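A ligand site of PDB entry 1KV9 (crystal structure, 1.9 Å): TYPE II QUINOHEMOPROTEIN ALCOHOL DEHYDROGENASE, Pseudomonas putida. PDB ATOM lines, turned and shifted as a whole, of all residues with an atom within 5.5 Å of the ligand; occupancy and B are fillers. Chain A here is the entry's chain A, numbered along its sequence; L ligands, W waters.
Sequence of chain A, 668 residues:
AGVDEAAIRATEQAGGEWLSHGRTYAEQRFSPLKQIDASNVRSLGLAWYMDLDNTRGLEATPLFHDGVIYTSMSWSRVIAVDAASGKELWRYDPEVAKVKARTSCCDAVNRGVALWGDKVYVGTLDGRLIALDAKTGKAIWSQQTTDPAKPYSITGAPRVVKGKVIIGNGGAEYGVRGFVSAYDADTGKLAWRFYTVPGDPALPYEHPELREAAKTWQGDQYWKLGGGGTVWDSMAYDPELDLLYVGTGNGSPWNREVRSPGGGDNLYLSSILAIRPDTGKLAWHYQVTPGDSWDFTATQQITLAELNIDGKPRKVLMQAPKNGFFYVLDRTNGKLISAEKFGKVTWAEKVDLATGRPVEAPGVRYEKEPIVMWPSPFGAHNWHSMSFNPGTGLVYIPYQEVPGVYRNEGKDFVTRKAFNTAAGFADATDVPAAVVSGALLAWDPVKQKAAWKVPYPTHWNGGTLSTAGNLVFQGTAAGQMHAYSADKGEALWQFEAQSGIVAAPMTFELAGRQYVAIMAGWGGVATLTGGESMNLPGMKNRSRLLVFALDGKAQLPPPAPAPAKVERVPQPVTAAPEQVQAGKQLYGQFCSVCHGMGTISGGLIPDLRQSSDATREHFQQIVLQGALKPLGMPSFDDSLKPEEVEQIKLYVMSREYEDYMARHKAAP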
ATOM      1  N   ARG A  56       7.280   8.641 -33.913  1.00  0.00           N
ATOM      2  CA  ARG A  56       7.833   8.274 -32.621  1.00  0.00           C
ATOM      3  C   ARG A  56       9.173   8.989 -32.422  1.00  0.00           C
ATOM      4  O   ARG A  56       9.595   9.770 -33.270  1.00  0.00           O
ATOM      5  CB  ARG A  56       8.006   6.749 -32.538  1.00  0.00           C
ATOM      6  CG  ARG A  56       6.674   5.989 -32.679  1.00  0.00           C
ATOM      7  CD  ARG A  56       5.725   6.283 -31.520  1.00  0.00           C
ATOM      8  NE  ARG A  56       6.199   5.701 -30.271  1.00  0.00           N
ATOM      9  CZ  ARG A  56       5.729   4.582 -29.743  1.00  0.00           C
ATOM     10  NH1 ARG A  56       4.756   3.912 -30.343  1.00  0.00           N
ATOM     11  NH2 ARG A  56       6.249   4.103 -28.613  1.00  0.00           N
ATOM     12  N   ALA A 101       7.388  -3.478 -29.203  1.00  0.00           N
ATOM     13  CA  ALA A 101       7.494  -2.379 -28.252  1.00  0.00           C
ATOM     14  C   ALA A 101       7.062  -2.807 -26.854  1.00  0.00           C
ATOM     15  O   ALA A 101       7.408  -2.151 -25.869  1.00  0.00           O
ATOM     16  CB  ALA A 101       6.658  -1.197 -28.726  1.00  0.00           C
ATOM     17  N   ARG A 102       6.299  -3.894 -26.764  1.00  0.00           N
ATOM     18  CA  ARG A 102       5.871  -4.375 -25.446  1.00  0.00           C
ATOM     19  C   ARG A 102       7.106  -4.766 -24.630  1.00  0.00           C
ATOM     20  O   ARG A 102       7.093  -4.722 -23.406  1.00  0.00           O
ATOM     21  CB  ARG A 102       4.927  -5.572 -25.563  1.00  0.00           C
ATOM     22  CG  ARG A 102       4.390  -6.031 -24.208  1.00  0.00           C
ATOM     23  CD  ARG A 102       3.485  -7.244 -24.283  1.00  0.00           C
ATOM     24  NE  ARG A 102       3.151  -7.730 -22.943  1.00  0.00           N
ATOM     25  CZ  ARG A 102       2.467  -8.829 -22.681  1.00  0.00           C
ATOM     26  NH1 ARG A 102       2.037  -9.600 -23.672  1.00  0.00           N
ATOM     27  NH2 ARG A 102       2.218  -9.187 -21.418  1.00  0.00           N
ATOM     28  N   TYR A 587      -3.065  -1.043 -13.976  1.00  0.00           N
ATOM     29  CA  TYR A 587      -2.732  -0.087 -15.027  1.00  0.00           C
ATOM     30  C   TYR A 587      -1.267   0.325 -14.910  1.00  0.00           C
ATOM     31  O   TYR A 587      -0.526   0.337 -15.888  1.00  0.00           O
ATOM     32  CB  TYR A 587      -3.611   1.161 -14.940  1.00  0.00           C
ATOM     33  CG  TYR A 587      -3.224   2.233 -15.935  1.00  0.00           C
ATOM     34  CD1 TYR A 587      -3.757   2.225 -17.237  1.00  0.00           C
ATOM     35  CD2 TYR A 587      -2.269   3.192 -15.627  1.00  0.00           C
ATOM     36  CE1 TYR A 587      -3.329   3.157 -18.189  1.00  0.00           C
ATOM     37  CE2 TYR A 587      -1.841   4.122 -16.565  1.00  0.00           C
ATOM     38  CZ  TYR A 587      -2.371   4.105 -17.847  1.00  0.00           C
ATOM     39  OH  TYR A 587      -1.914   5.001 -18.776  1.00  0.00           O
ATOM     40  N   PHE A 590       1.061  -2.657 -16.011  1.00  0.00           N
ATOM     41  CA  PHE A 590       1.030  -3.073 -17.417  1.00  0.00           C
ATOM     42  C   PHE A 590       0.817  -2.029 -18.501  1.00  0.00           C
ATOM     43  O   PHE A 590       1.228  -2.239 -19.636  1.00  0.00           O
ATOM     44  CB  PHE A 590      -0.050  -4.141 -17.602  1.00  0.00           C
ATOM     45  CG  PHE A 590       0.250  -5.440 -16.915  1.00  0.00           C
ATOM     46  CD1 PHE A 590       1.009  -6.413 -17.549  1.00  0.00           C
ATOM     47  CD2 PHE A 590      -0.219  -5.684 -15.624  1.00  0.00           C
ATOM     48  CE1 PHE A 590       1.305  -7.616 -16.911  1.00  0.00           C
ATOM     49  CE2 PHE A 590       0.065  -6.886 -14.979  1.00  0.00           C
ATOM     50  CZ  PHE A 590       0.830  -7.847 -15.618  1.00  0.00           C
ATOM     51  N   CYS A 591       0.176  -0.899 -18.176  1.00  0.00           N
ATOM     52  CA  CYS A 591      -0.120   0.082 -19.222  1.00  0.00           C
ATOM     53  C   CYS A 591       0.576   1.440 -19.171  1.00  0.00           C
ATOM     54  O   CYS A 591       0.761   2.067 -20.213  1.00  0.00           O
ATOM     55  CB  CYS A 591      -1.635   0.325 -19.265  1.00  0.00           C
ATOM     56  SG  CYS A 591      -2.659  -1.124 -18.829  1.00  0.00           S
ATOM     57  N   VAL A 593       3.591   2.420 -18.931  1.00  0.00           N
ATOM     58  CA  VAL A 593       4.808   2.595 -19.723  1.00  0.00           C
ATOM     59  C   VAL A 593       4.591   3.051 -21.166  1.00  0.00           C
ATOM     60  O   VAL A 593       5.541   3.465 -21.839  1.00  0.00           O
ATOM     61  CB  VAL A 593       5.666   1.305 -19.718  1.00  0.00           C
ATOM     62  CG1 VAL A 593       6.061   0.964 -18.288  1.00  0.00           C
ATOM     63  CG2 VAL A 593       4.915   0.161 -20.374  1.00  0.00           C
ATOM     64  N   CYS A 594       3.355   2.994 -21.637  1.00  0.00           N
ATOM     65  CA  CYS A 594       3.043   3.438 -22.991  1.00  0.00           C
ATOM     66  C   CYS A 594       1.921   4.480 -22.991  1.00  0.00           C
ATOM     67  O   CYS A 594       1.973   5.443 -23.746  1.00  0.00           O
ATOM     68  CB  CYS A 594       2.651   2.261 -23.888  1.00  0.00           C
ATOM     69  SG  CYS A 594       4.013   1.166 -24.415  1.00  0.00           S
ATOM     70  N   HIS A 595       0.915   4.289 -22.140  1.00  0.00           N
ATOM     71  CA  HIS A 595      -0.203   5.235 -22.091  1.00  0.00           C
ATOM     72  C   HIS A 595      -0.047   6.351 -21.050  1.00  0.00           C
ATOM     73  O   HIS A 595      -0.922   7.223 -20.929  1.00  0.00           O
ATOM     74  CB  HIS A 595      -1.510   4.464 -21.883  1.00  0.00           C
ATOM     75  CG  HIS A 595      -1.968   3.727 -23.112  1.00  0.00           C
ATOM     76  ND1 HIS A 595      -2.476   4.394 -24.177  1.00  0.00           N
ATOM     77  CD2 HIS A 595      -1.839   2.384 -23.152  1.00  0.00           C
ATOM     78  CE1 HIS A 595      -2.705   3.353 -25.057  1.00  0.00           C
ATOM     79  NE2 HIS A 595      -2.322   2.105 -24.438  1.00  0.00           N
ATOM     80  N   ILE A 605       1.236   8.134 -27.887  1.00  0.00           N
ATOM     81  CA  ILE A 605       0.301   7.008 -27.828  1.00  0.00           C
ATOM     82  C   ILE A 605      -0.990   7.560 -27.208  1.00  0.00           C
ATOM     83  O   ILE A 605      -0.939   8.403 -26.314  1.00  0.00           O
ATOM     84  CB  ILE A 605       0.910   5.883 -26.964  1.00  0.00           C
ATOM     85  CG1 ILE A 605       2.189   5.364 -27.636  1.00  0.00           C
ATOM     86  CG2 ILE A 605      -0.108   4.753 -26.764  1.00  0.00           C
ATOM     87  CD1 ILE A 605       2.972   4.352 -26.836  1.00  0.00           C
ATOM     88  N   PRO A 606      -2.158   7.103 -27.678  1.00  0.00           N
ATOM     89  CA  PRO A 606      -3.467   7.550 -27.203  1.00  0.00           C
ATOM     90  C   PRO A 606      -3.681   7.691 -25.703  1.00  0.00           C
ATOM     91  O   PRO A 606      -3.187   6.896 -24.896  1.00  0.00           O
ATOM     92  CB  PRO A 606      -4.417   6.524 -27.824  1.00  0.00           C
ATOM     93  CG  PRO A 606      -3.764   6.204 -29.107  1.00  0.00           C
ATOM     94  CD  PRO A 606      -2.311   6.034 -28.682  1.00  0.00           C
ATOM     95  N   ASP A 607      -4.454   8.721 -25.340  1.00  0.00           N
ATOM     96  CA  ASP A 607      -4.811   9.011 -23.962  1.00  0.00           C
ATOM     97  C   ASP A 607      -6.094   8.228 -23.698  1.00  0.00           C
ATOM     98  O   ASP A 607      -7.164   8.557 -24.219  1.00  0.00           O
ATOM     99  CB  ASP A 607      -5.061  10.521 -23.805  1.00  0.00           C
ATOM    100  CG  ASP A 607      -5.466  10.911 -22.398  1.00  0.00           C
ATOM    101  OD1 ASP A 607      -5.553  12.138 -22.139  1.00  0.00           O
ATOM    102  OD2 ASP A 607      -5.701  10.025 -21.548  1.00  0.00           O
ATOM    103  N   LEU A 608      -5.983   7.174 -22.896  1.00  0.00           N
ATOM    104  CA  LEU A 608      -7.129   6.325 -22.590  1.00  0.00           C
ATOM    105  C   LEU A 608      -8.305   7.078 -21.964  1.00  0.00           C
ATOM    106  O   LEU A 608      -9.419   6.570 -21.932  1.00  0.00           O
ATOM    107  CB  LEU A 608      -6.703   5.169 -21.691  1.00  0.00           C
ATOM    108  CG  LEU A 608      -5.603   4.259 -22.279  1.00  0.00           C
ATOM    109  CD1 LEU A 608      -5.532   2.974 -21.480  1.00  0.00           C
ATOM    110  CD2 LEU A 608      -5.920   3.946 -23.732  1.00  0.00           C
ATOM    111  N   GLN A 610      -9.422   9.810 -23.134  1.00  0.00           N
ATOM    112  CA  GLN A 610     -10.142  10.396 -24.273  1.00  0.00           C
ATOM    113  C   GLN A 610     -10.685   9.405 -25.295  1.00  0.00           C
ATOM    114  O   GLN A 610     -11.203   9.823 -26.334  1.00  0.00           O
ATOM    115  CB  GLN A 610      -9.238  11.401 -24.982  1.00  0.00           C
ATOM    116  CG  GLN A 610      -8.781  12.571 -24.113  1.00  0.00           C
ATOM    117  CD  GLN A 610      -9.942  13.345 -23.520  1.00  0.00           C
ATOM    118  OE1 GLN A 610     -10.865  13.756 -24.225  1.00  0.00           O
ATOM    119  NE2 GLN A 610      -9.900  13.556 -22.196  1.00  0.00           N
ATOM    120  N   SER A 611     -10.559   8.108 -25.033  1.00  0.00           N
ATOM    121  CA  SER A 611     -11.046   7.103 -25.970  1.00  0.00           C
ATOM    122  C   SER A 611     -12.509   7.316 -26.324  1.00  0.00           C
ATOM    123  O   SER A 611     -13.304   7.748 -25.484  1.00  0.00           O
ATOM    124  CB  SER A 611     -10.870   5.697 -25.388  1.00  0.00           C
ATOM    125  OG  SER A 611      -9.497   5.389 -25.194  1.00  0.00           O
ATOM    126  N   SER A 612     -12.871   7.020 -27.568  1.00  0.00           N
ATOM    127  CA  SER A 612     -14.243   7.176 -28.022  1.00  0.00           C
ATOM    128  C   SER A 612     -15.120   6.113 -27.364  1.00  0.00           C
ATOM    129  O   SER A 612     -14.603   5.177 -26.751  1.00  0.00           O
ATOM    130  CB  SER A 612     -14.333   7.025 -29.545  1.00  0.00           C
ATOM    131  OG  SER A 612     -13.982   5.708 -29.941  1.00  0.00           O
ATOM    132  N   THR A 615     -14.560   2.699 -28.878  1.00  0.00           N
ATOM    133  CA  THR A 615     -13.323   2.120 -28.351  1.00  0.00           C
ATOM    134  C   THR A 615     -13.559   1.494 -26.966  1.00  0.00           C
ATOM    135  O   THR A 615     -13.122   0.380 -26.697  1.00  0.00           O
ATOM    136  CB  THR A 615     -12.214   3.192 -28.243  1.00  0.00           C
ATOM    137  OG1 THR A 615     -11.802   3.580 -29.562  1.00  0.00           O
ATOM    138  CG2 THR A 615     -11.004   2.652 -27.473  1.00  0.00           C
ATOM    139  N   PHE A 619     -13.062  -2.446 -25.435  1.00  0.00           N
ATOM    140  CA  PHE A 619     -11.930  -2.456 -24.525  1.00  0.00           C
ATOM    141  C   PHE A 619     -11.367  -3.875 -24.324  1.00  0.00           C
ATOM    142  O   PHE A 619     -10.163  -4.080 -24.390  1.00  0.00           O
ATOM    143  CB  PHE A 619     -12.340  -1.844 -23.183  1.00  0.00           C
ATOM    144  CG  PHE A 619     -11.205  -1.273 -22.381  1.00  0.00           C
ATOM    145  CD1 PHE A 619     -10.572  -2.021 -21.398  1.00  0.00           C
ATOM    146  CD2 PHE A 619     -10.770   0.029 -22.608  1.00  0.00           C
ATOM    147  CE1 PHE A 619      -9.527  -1.488 -20.640  1.00  0.00           C
ATOM    148  CE2 PHE A 619      -9.719   0.576 -21.869  1.00  0.00           C
ATOM    149  CZ  PHE A 619      -9.103  -0.181 -20.889  1.00  0.00           C
ATOM    150  N   ILE A 622      -9.717  -5.174 -27.599  1.00  0.00           N
ATOM    151  CA  ILE A 622      -8.426  -4.532 -27.835  1.00  0.00           C
ATOM    152  C   ILE A 622      -7.345  -5.078 -26.918  1.00  0.00           C
ATOM    153  O   ILE A 622      -6.291  -5.531 -27.370  1.00  0.00           O
ATOM    154  CB  ILE A 622      -8.515  -3.007 -27.636  1.00  0.00           C
ATOM    155  CG1 ILE A 622      -9.400  -2.385 -28.723  1.00  0.00           C
ATOM    156  CG2 ILE A 622      -7.117  -2.394 -27.639  1.00  0.00           C
ATOM    157  CD1 ILE A 622      -9.729  -0.933 -28.491  1.00  0.00           C
ATOM    158  N   VAL A 623      -7.611  -5.031 -25.613  1.00  0.00           N
ATOM    159  CA  VAL A 623      -6.659  -5.454 -24.594  1.00  0.00           C
ATOM    160  C   VAL A 623      -6.377  -6.950 -24.490  1.00  0.00           C
ATOM    161  O   VAL A 623      -5.233  -7.351 -24.258  1.00  0.00           O
ATOM    162  CB  VAL A 623      -7.094  -4.929 -23.208  1.00  0.00           C
ATOM    163  CG1 VAL A 623      -6.065  -5.312 -22.152  1.00  0.00           C
ATOM    164  CG2 VAL A 623      -7.281  -3.426 -23.259  1.00  0.00           C
ATOM    165  N   LEU A 628      -6.139  -4.376 -31.960  1.00  0.00           N
ATOM    166  CA  LEU A 628      -5.296  -3.302 -32.487  1.00  0.00           C
ATOM    167  C   LEU A 628      -3.828  -3.720 -32.574  1.00  0.00           C
ATOM    168  O   LEU A 628      -2.934  -2.881 -32.651  1.00  0.00           O
ATOM    169  CB  LEU A 628      -5.430  -2.051 -31.617  1.00  0.00           C
ATOM    170  CG  LEU A 628      -6.382  -0.936 -32.054  1.00  0.00           C
ATOM    171  CD1 LEU A 628      -7.574  -1.497 -32.812  1.00  0.00           C
ATOM    172  CD2 LEU A 628      -6.835  -0.166 -30.830  1.00  0.00           C
ATOM    173  N   LEU A 631      -1.421  -2.363 -35.144  1.00  0.00           N
ATOM    174  CA  LEU A 631      -1.027  -0.975 -34.936  1.00  0.00           C
ATOM    175  C   LEU A 631      -0.016  -0.859 -33.794  1.00  0.00           C
ATOM    176  O   LEU A 631       0.458   0.228 -33.475  1.00  0.00           O
ATOM    177  CB  LEU A 631      -2.258  -0.127 -34.626  1.00  0.00           C
ATOM    178  CG  LEU A 631      -3.299  -0.073 -35.749  1.00  0.00           C
ATOM    179  CD1 LEU A 631      -4.482   0.769 -35.310  1.00  0.00           C
ATOM    180  CD2 LEU A 631      -2.665   0.521 -37.002  1.00  0.00           C
ATOM    181  N   GLY A 632       0.311  -1.992 -33.173  1.00  0.00           N
ATOM    182  CA  GLY A 632       1.281  -1.974 -32.090  1.00  0.00           C
ATOM    183  C   GLY A 632       0.727  -2.111 -30.691  1.00  0.00           C
ATOM    184  O   GLY A 632       1.493  -2.180 -29.726  1.00  0.00           O
ATOM    185  N   MET A 633      -0.594  -2.119 -30.548  1.00  0.00           N
ATOM    186  CA  MET A 633      -1.223  -2.270 -29.238  1.00  0.00           C
ATOM    187  C   MET A 633      -1.253  -3.761 -28.968  1.00  0.00           C
ATOM    188  O   MET A 633      -2.047  -4.499 -29.567  1.00  0.00           O
ATOM    189  CB  MET A 633      -2.635  -1.688 -29.253  1.00  0.00           C
ATOM    190  CG  MET A 633      -3.484  -2.022 -28.035  1.00  0.00           C
ATOM    191  SD  MET A 633      -2.695  -1.836 -26.406  1.00  0.00           S
ATOM    192  CE  MET A 633      -3.686  -3.015 -25.476  1.00  0.00           C
ATOM    193  N   PRO A 634      -0.395  -4.239 -28.060  1.00  0.00           N
ATOM    194  CA  PRO A 634      -0.300  -5.660 -27.711  1.00  0.00           C
ATOM    195  C   PRO A 634      -1.556  -6.242 -27.064  1.00  0.00           C
ATOM    196  O   PRO A 634      -2.405  -5.510 -26.563  1.00  0.00           O
ATOM    197  CB  PRO A 634       0.881  -5.709 -26.728  1.00  0.00           C
ATOM    198  CG  PRO A 634       1.631  -4.423 -26.987  1.00  0.00           C
ATOM    199  CD  PRO A 634       0.529  -3.450 -27.227  1.00  0.00           C
ATOM    200  N   PHE A 636      -2.860  -8.593 -24.049  1.00  0.00           N
ATOM    201  CA  PHE A 636      -2.341  -9.022 -22.760  1.00  0.00           C
ATOM    202  C   PHE A 636      -3.061 -10.238 -22.188  1.00  0.00           C
ATOM    203  O   PHE A 636      -3.125 -10.405 -20.970  1.00  0.00           O
ATOM    204  CB  PHE A 636      -2.431  -7.875 -21.741  1.00  0.00           C
ATOM    205  CG  PHE A 636      -1.576  -6.694 -22.101  1.00  0.00           C
ATOM    206  CD1 PHE A 636      -1.952  -5.823 -23.116  1.00  0.00           C
ATOM    207  CD2 PHE A 636      -0.364  -6.471 -21.439  1.00  0.00           C
ATOM    208  CE1 PHE A 636      -1.138  -4.749 -23.480  1.00  0.00           C
ATOM    209  CE2 PHE A 636       0.450  -5.400 -21.789  1.00  0.00           C
ATOM    210  CZ  PHE A 636       0.056  -4.538 -22.805  1.00  0.00           C
ATOM    211  N   LEU A 640      -3.382 -10.925 -18.186  1.00  0.00           N
ATOM    212  CA  LEU A 640      -4.563 -10.369 -17.542  1.00  0.00           C
ATOM    213  C   LEU A 640      -5.874 -11.093 -17.849  1.00  0.00           C
ATOM    214  O   LEU A 640      -6.082 -11.582 -18.963  1.00  0.00           O
ATOM    215  CB  LEU A 640      -4.697  -8.892 -17.932  1.00  0.00           C
ATOM    216  CG  LEU A 640      -3.491  -8.012 -17.595  1.00  0.00           C
ATOM    217  CD1 LEU A 640      -3.645  -6.637 -18.210  1.00  0.00           C
ATOM    218  CD2 LEU A 640      -3.349  -7.910 -16.079  1.00  0.00           C
ATOM    219  N   VAL A 645      -9.020  -6.578 -16.607  1.00  0.00           N
ATOM    220  CA  VAL A 645      -9.053  -5.536 -17.630  1.00  0.00           C
ATOM    221  C   VAL A 645     -10.205  -4.582 -17.323  1.00  0.00           C
ATOM    222  O   VAL A 645     -10.115  -3.383 -17.560  1.00  0.00           O
ATOM    223  CB  VAL A 645      -9.231  -6.138 -19.041  1.00  0.00           C
ATOM    224  CG1 VAL A 645      -9.518  -5.040 -20.053  1.00  0.00           C
ATOM    225  CG2 VAL A 645      -7.975  -6.893 -19.436  1.00  0.00           C
ATOM    226  N   ILE A 648      -9.206  -2.158 -14.796  1.00  0.00           N
ATOM    227  CA  ILE A 648      -8.374  -1.129 -15.403  1.00  0.00           C
ATOM    228  C   ILE A 648      -9.262  -0.082 -16.070  1.00  0.00           C
ATOM    229  O   ILE A 648      -9.059   1.126 -15.917  1.00  0.00           O
ATOM    230  CB  ILE A 648      -7.408  -1.734 -16.460  1.00  0.00           C
ATOM    231  CG1 ILE A 648      -6.380  -2.629 -15.758  1.00  0.00           C
ATOM    232  CG2 ILE A 648      -6.695  -0.628 -17.222  1.00  0.00           C
ATOM    233  CD1 ILE A 648      -5.429  -3.350 -16.713  1.00  0.00           C
HETATM  234 FE1  LIG L   1      -2.487   0.289 -25.426  1.00  0.00          FE
HETATM  235  C1  LIG L   1      -4.039   1.839 -28.018  1.00  0.00           C
HETATM  236  C2  LIG L   1      -5.493  -0.078 -23.834  1.00  0.00           C
HETATM  237  C3  LIG L   1      -0.925  -1.190 -22.772  1.00  0.00           C
HETATM  238  C4  LIG L   1       0.534   0.749 -26.916  1.00  0.00           C
HETATM  239  N1  LIG L   1      -4.421   0.772 -25.854  1.00  0.00           N
HETATM  240  C5  LIG L   1      -4.853   1.420 -26.985  1.00  0.00           C
HETATM  241  C6  LIG L   1      -6.306   1.590 -26.901  1.00  0.00           C
HETATM  242  C7  LIG L   1      -6.705   1.050 -25.735  1.00  0.00           C
HETATM  243  C8  LIG L   1      -5.533   0.535 -25.063  1.00  0.00           C
HETATM  244  C9  LIG L   1      -8.133   0.983 -25.174  1.00  0.00           C
HETATM  245  C10 LIG L   1      -7.154   2.305 -27.965  1.00  0.00           C
HETATM  246  C11 LIG L   1      -7.041   3.815 -27.636  1.00  0.00           C
HETATM  247  C12 LIG L   1      -7.900   4.795 -28.414  1.00  0.00           C
HETATM  248  O1  LIG L   1      -7.743   4.769 -29.683  1.00  0.00           O
HETATM  249  O2  LIG L   1      -8.650   5.552 -27.793  1.00  0.00           O
HETATM  250  N2  LIG L   1      -3.075  -0.486 -23.656  1.00  0.00           N
HETATM  251  C13 LIG L   1      -4.382  -0.543 -23.184  1.00  0.00           C
HETATM  252  C14 LIG L   1      -4.404  -1.164 -21.865  1.00  0.00           C
HETATM  253  C15 LIG L   1      -3.110  -1.475 -21.580  1.00  0.00           C
HETATM  254  C16 LIG L   1      -2.292  -1.069 -22.680  1.00  0.00           C
HETATM  255  C17 LIG L   1      -5.652  -1.399 -21.012  1.00  0.00           C
HETATM  256  C18 LIG L   1      -2.550  -2.148 -20.322  1.00  0.00           C
HETATM  257  C19 LIG L   1      -2.950  -3.621 -20.150  1.00  0.00           C
HETATM  258  N3  LIG L   1      -0.586  -0.145 -24.955  1.00  0.00           N
HETATM  259  C20 LIG L   1      -0.130  -0.756 -23.811  1.00  0.00           C
HETATM  260  C21 LIG L   1       1.323  -0.863 -23.819  1.00  0.00           C
HETATM  261  C22 LIG L   1       1.739  -0.317 -24.956  1.00  0.00           C
HETATM  262  C23 LIG L   1       0.558   0.127 -25.690  1.00  0.00           C
HETATM  263  C24 LIG L   1       2.167  -1.487 -22.662  1.00  0.00           C
HETATM  264  C25 LIG L   1       3.174  -0.113 -25.459  1.00  0.00           C
HETATM  265  C26 LIG L   1       3.996  -1.382 -25.752  1.00  0.00           C
HETATM  266  N4  LIG L   1      -1.884   1.103 -27.124  1.00  0.00           N
HETATM  267  C27 LIG L   1      -0.574   1.196 -27.605  1.00  0.00           C
HETATM  268  C28 LIG L   1      -0.560   1.867 -28.895  1.00  0.00           C
HETATM  269  C29 LIG L   1      -1.842   2.179 -29.201  1.00  0.00           C
HETATM  270  C30 LIG L   1      -2.665   1.703 -28.097  1.00  0.00           C
HETATM  271  C31 LIG L   1       0.713   2.153 -29.718  1.00  0.00           C
HETATM  272  C32 LIG L   1      -2.325   2.924 -30.467  1.00  0.00           C
HETATM  273  C33 LIG L   1      -2.637   2.034 -31.697  1.00  0.00           C
HETATM  274  C34 LIG L   1      -3.071   2.932 -32.844  1.00  0.00           C
HETATM  275  O3  LIG L   1      -2.345   3.052 -33.834  1.00  0.00           O
HETATM  276  O4  LIG L   1      -4.165   3.513 -32.696  1.00  0.00           O
HETATM  277  O   HOH W   1       5.298  -2.812 -22.272  1.00  0.00           O
HETATM  278  O   HOH W   2      -6.106   3.322 -31.054  1.00  0.00           O
HETATM  279  O   HOH W   3       0.228   2.740 -34.189  1.00  0.00           O
HETATM  280  O   HOH W   4     -10.747   6.140 -29.369  1.00  0.00           O
HETATM  281  O   HOH W   5      -7.087   7.102 -31.074  1.00  0.00           O
HETATM  282  O   HOH W   6      -7.733   8.129 -26.977  1.00  0.00           O
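The side-chain sulfur of Cys 591 is bonded to a carbon (C18) of the ligand, 1.8 Å away. A carbon (C25) of the ligand is bonded to the side-chain sulfur (SG) of Cys 594, at 1.9 Å. An iron atom (FE1) of the ligand is bound by a ring nitrogen (NE2) of His 595 (2.1 Å). SD of Met 633 binds FE1 of the ligand, at 2.3 Å. An oxygen (O2) of the ligand is in hydrogen-bond range of the side-chain hydroxyl (OG) of Ser 611 (2.7 Å).
A ring nitrogen (ND1) of His 595 sits at hydrogen-bond distance from the backbone carbonyl oxygen (O) of Pro 606 (2.7 Å). The backbone carbonyl oxygen (O) of His 595 sits close to the side-chain hydroxyl (OH) of Tyr 587 (3.2 Å). The backbone NH (N) of Met 633 sits at hydrogen-bond distance from the backbone carbonyl oxygen (O) of Leu 628 (3.2 Å). The side-chain hydroxyl (OG) of Ser 611 sits at hydrogen-bond distance from the backbone carbonyl oxygen (O) of Leu 608 (3.5 Å). O of Val 623 sits at hydrogen-bond distance from N of Phe 636 (2.7 Å). The side-chain hydroxyl (OG) of Ser 612 is in hydrogen-bond range of the side-chain hydroxyl (OG1) of Thr 615.
Ala 101 touches the ligand. CA of Arg 102 touches C26 of the ligand, at 3.5 Å. Phe 590 touches the ligand. Val 593 touches the ligand. Ile 605 touches the ligand. Pro 606 touches the ligand. Leu 608 touches the ligand. CG2 of Thr 615 touches O2 of the ligand, at 3.7 Å. Phe 619 touches the ligand. Ile 622 touches the ligand (CG2 to C7, 3.96 Å). CG2 of Val 623 touches C17 of the ligand, at 3.4 Å. Leu 628 touches the ligand. Leu 631 touches the ligand. Pro 634 touches the ligand. CZ of Phe 636 touches C3 of the ligand, at 3.5 Å. Leu 640 touches the ligand. Hydrophobic or aromatic side chains that line the ligand: Ala 101, Phe 590, Val 593, His 595, Ile 605, Pro 606, Leu 608, Phe 619, Ile 622, Val 623, Leu 628, Leu 631, Met 633, Pro 634, Phe 636 and Leu 640. Within 4 Å of the ligand: Ala 101, Arg 102, Phe 590, Cys 591, Val 593, Cys 594, His 595, Ile 605, Pro 606, Leu 608, Ser 611, Thr 615, Phe 619, Ile 622, Val 623, Leu 628, Leu 631, Met 633, Pro 634, Phe 636 and Leu 640. The nearest printed residue that does not touch the ligand is Ile 648 (4.01 Å).
Water W3 bridges O3 of the ligand (2.6 Å) and O of Leu 631 (2.6 Å). Water W4 lies within hydrogen-bond range of an oxygen (O2) of the ligand (2.7 Å), the side-chain hydroxyl of Thr 615 (2.8 Å) and the backbone NH of Ser 612 (2.9 Å). Water W6 lies within hydrogen-bond range of the backbone carbonyl oxygen (O) of Asp 607 (2.8 Å), an oxygen (O2) of the ligand (2.9 Å) and the backbone NH (N) of Ser 611 (3.4 Å).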
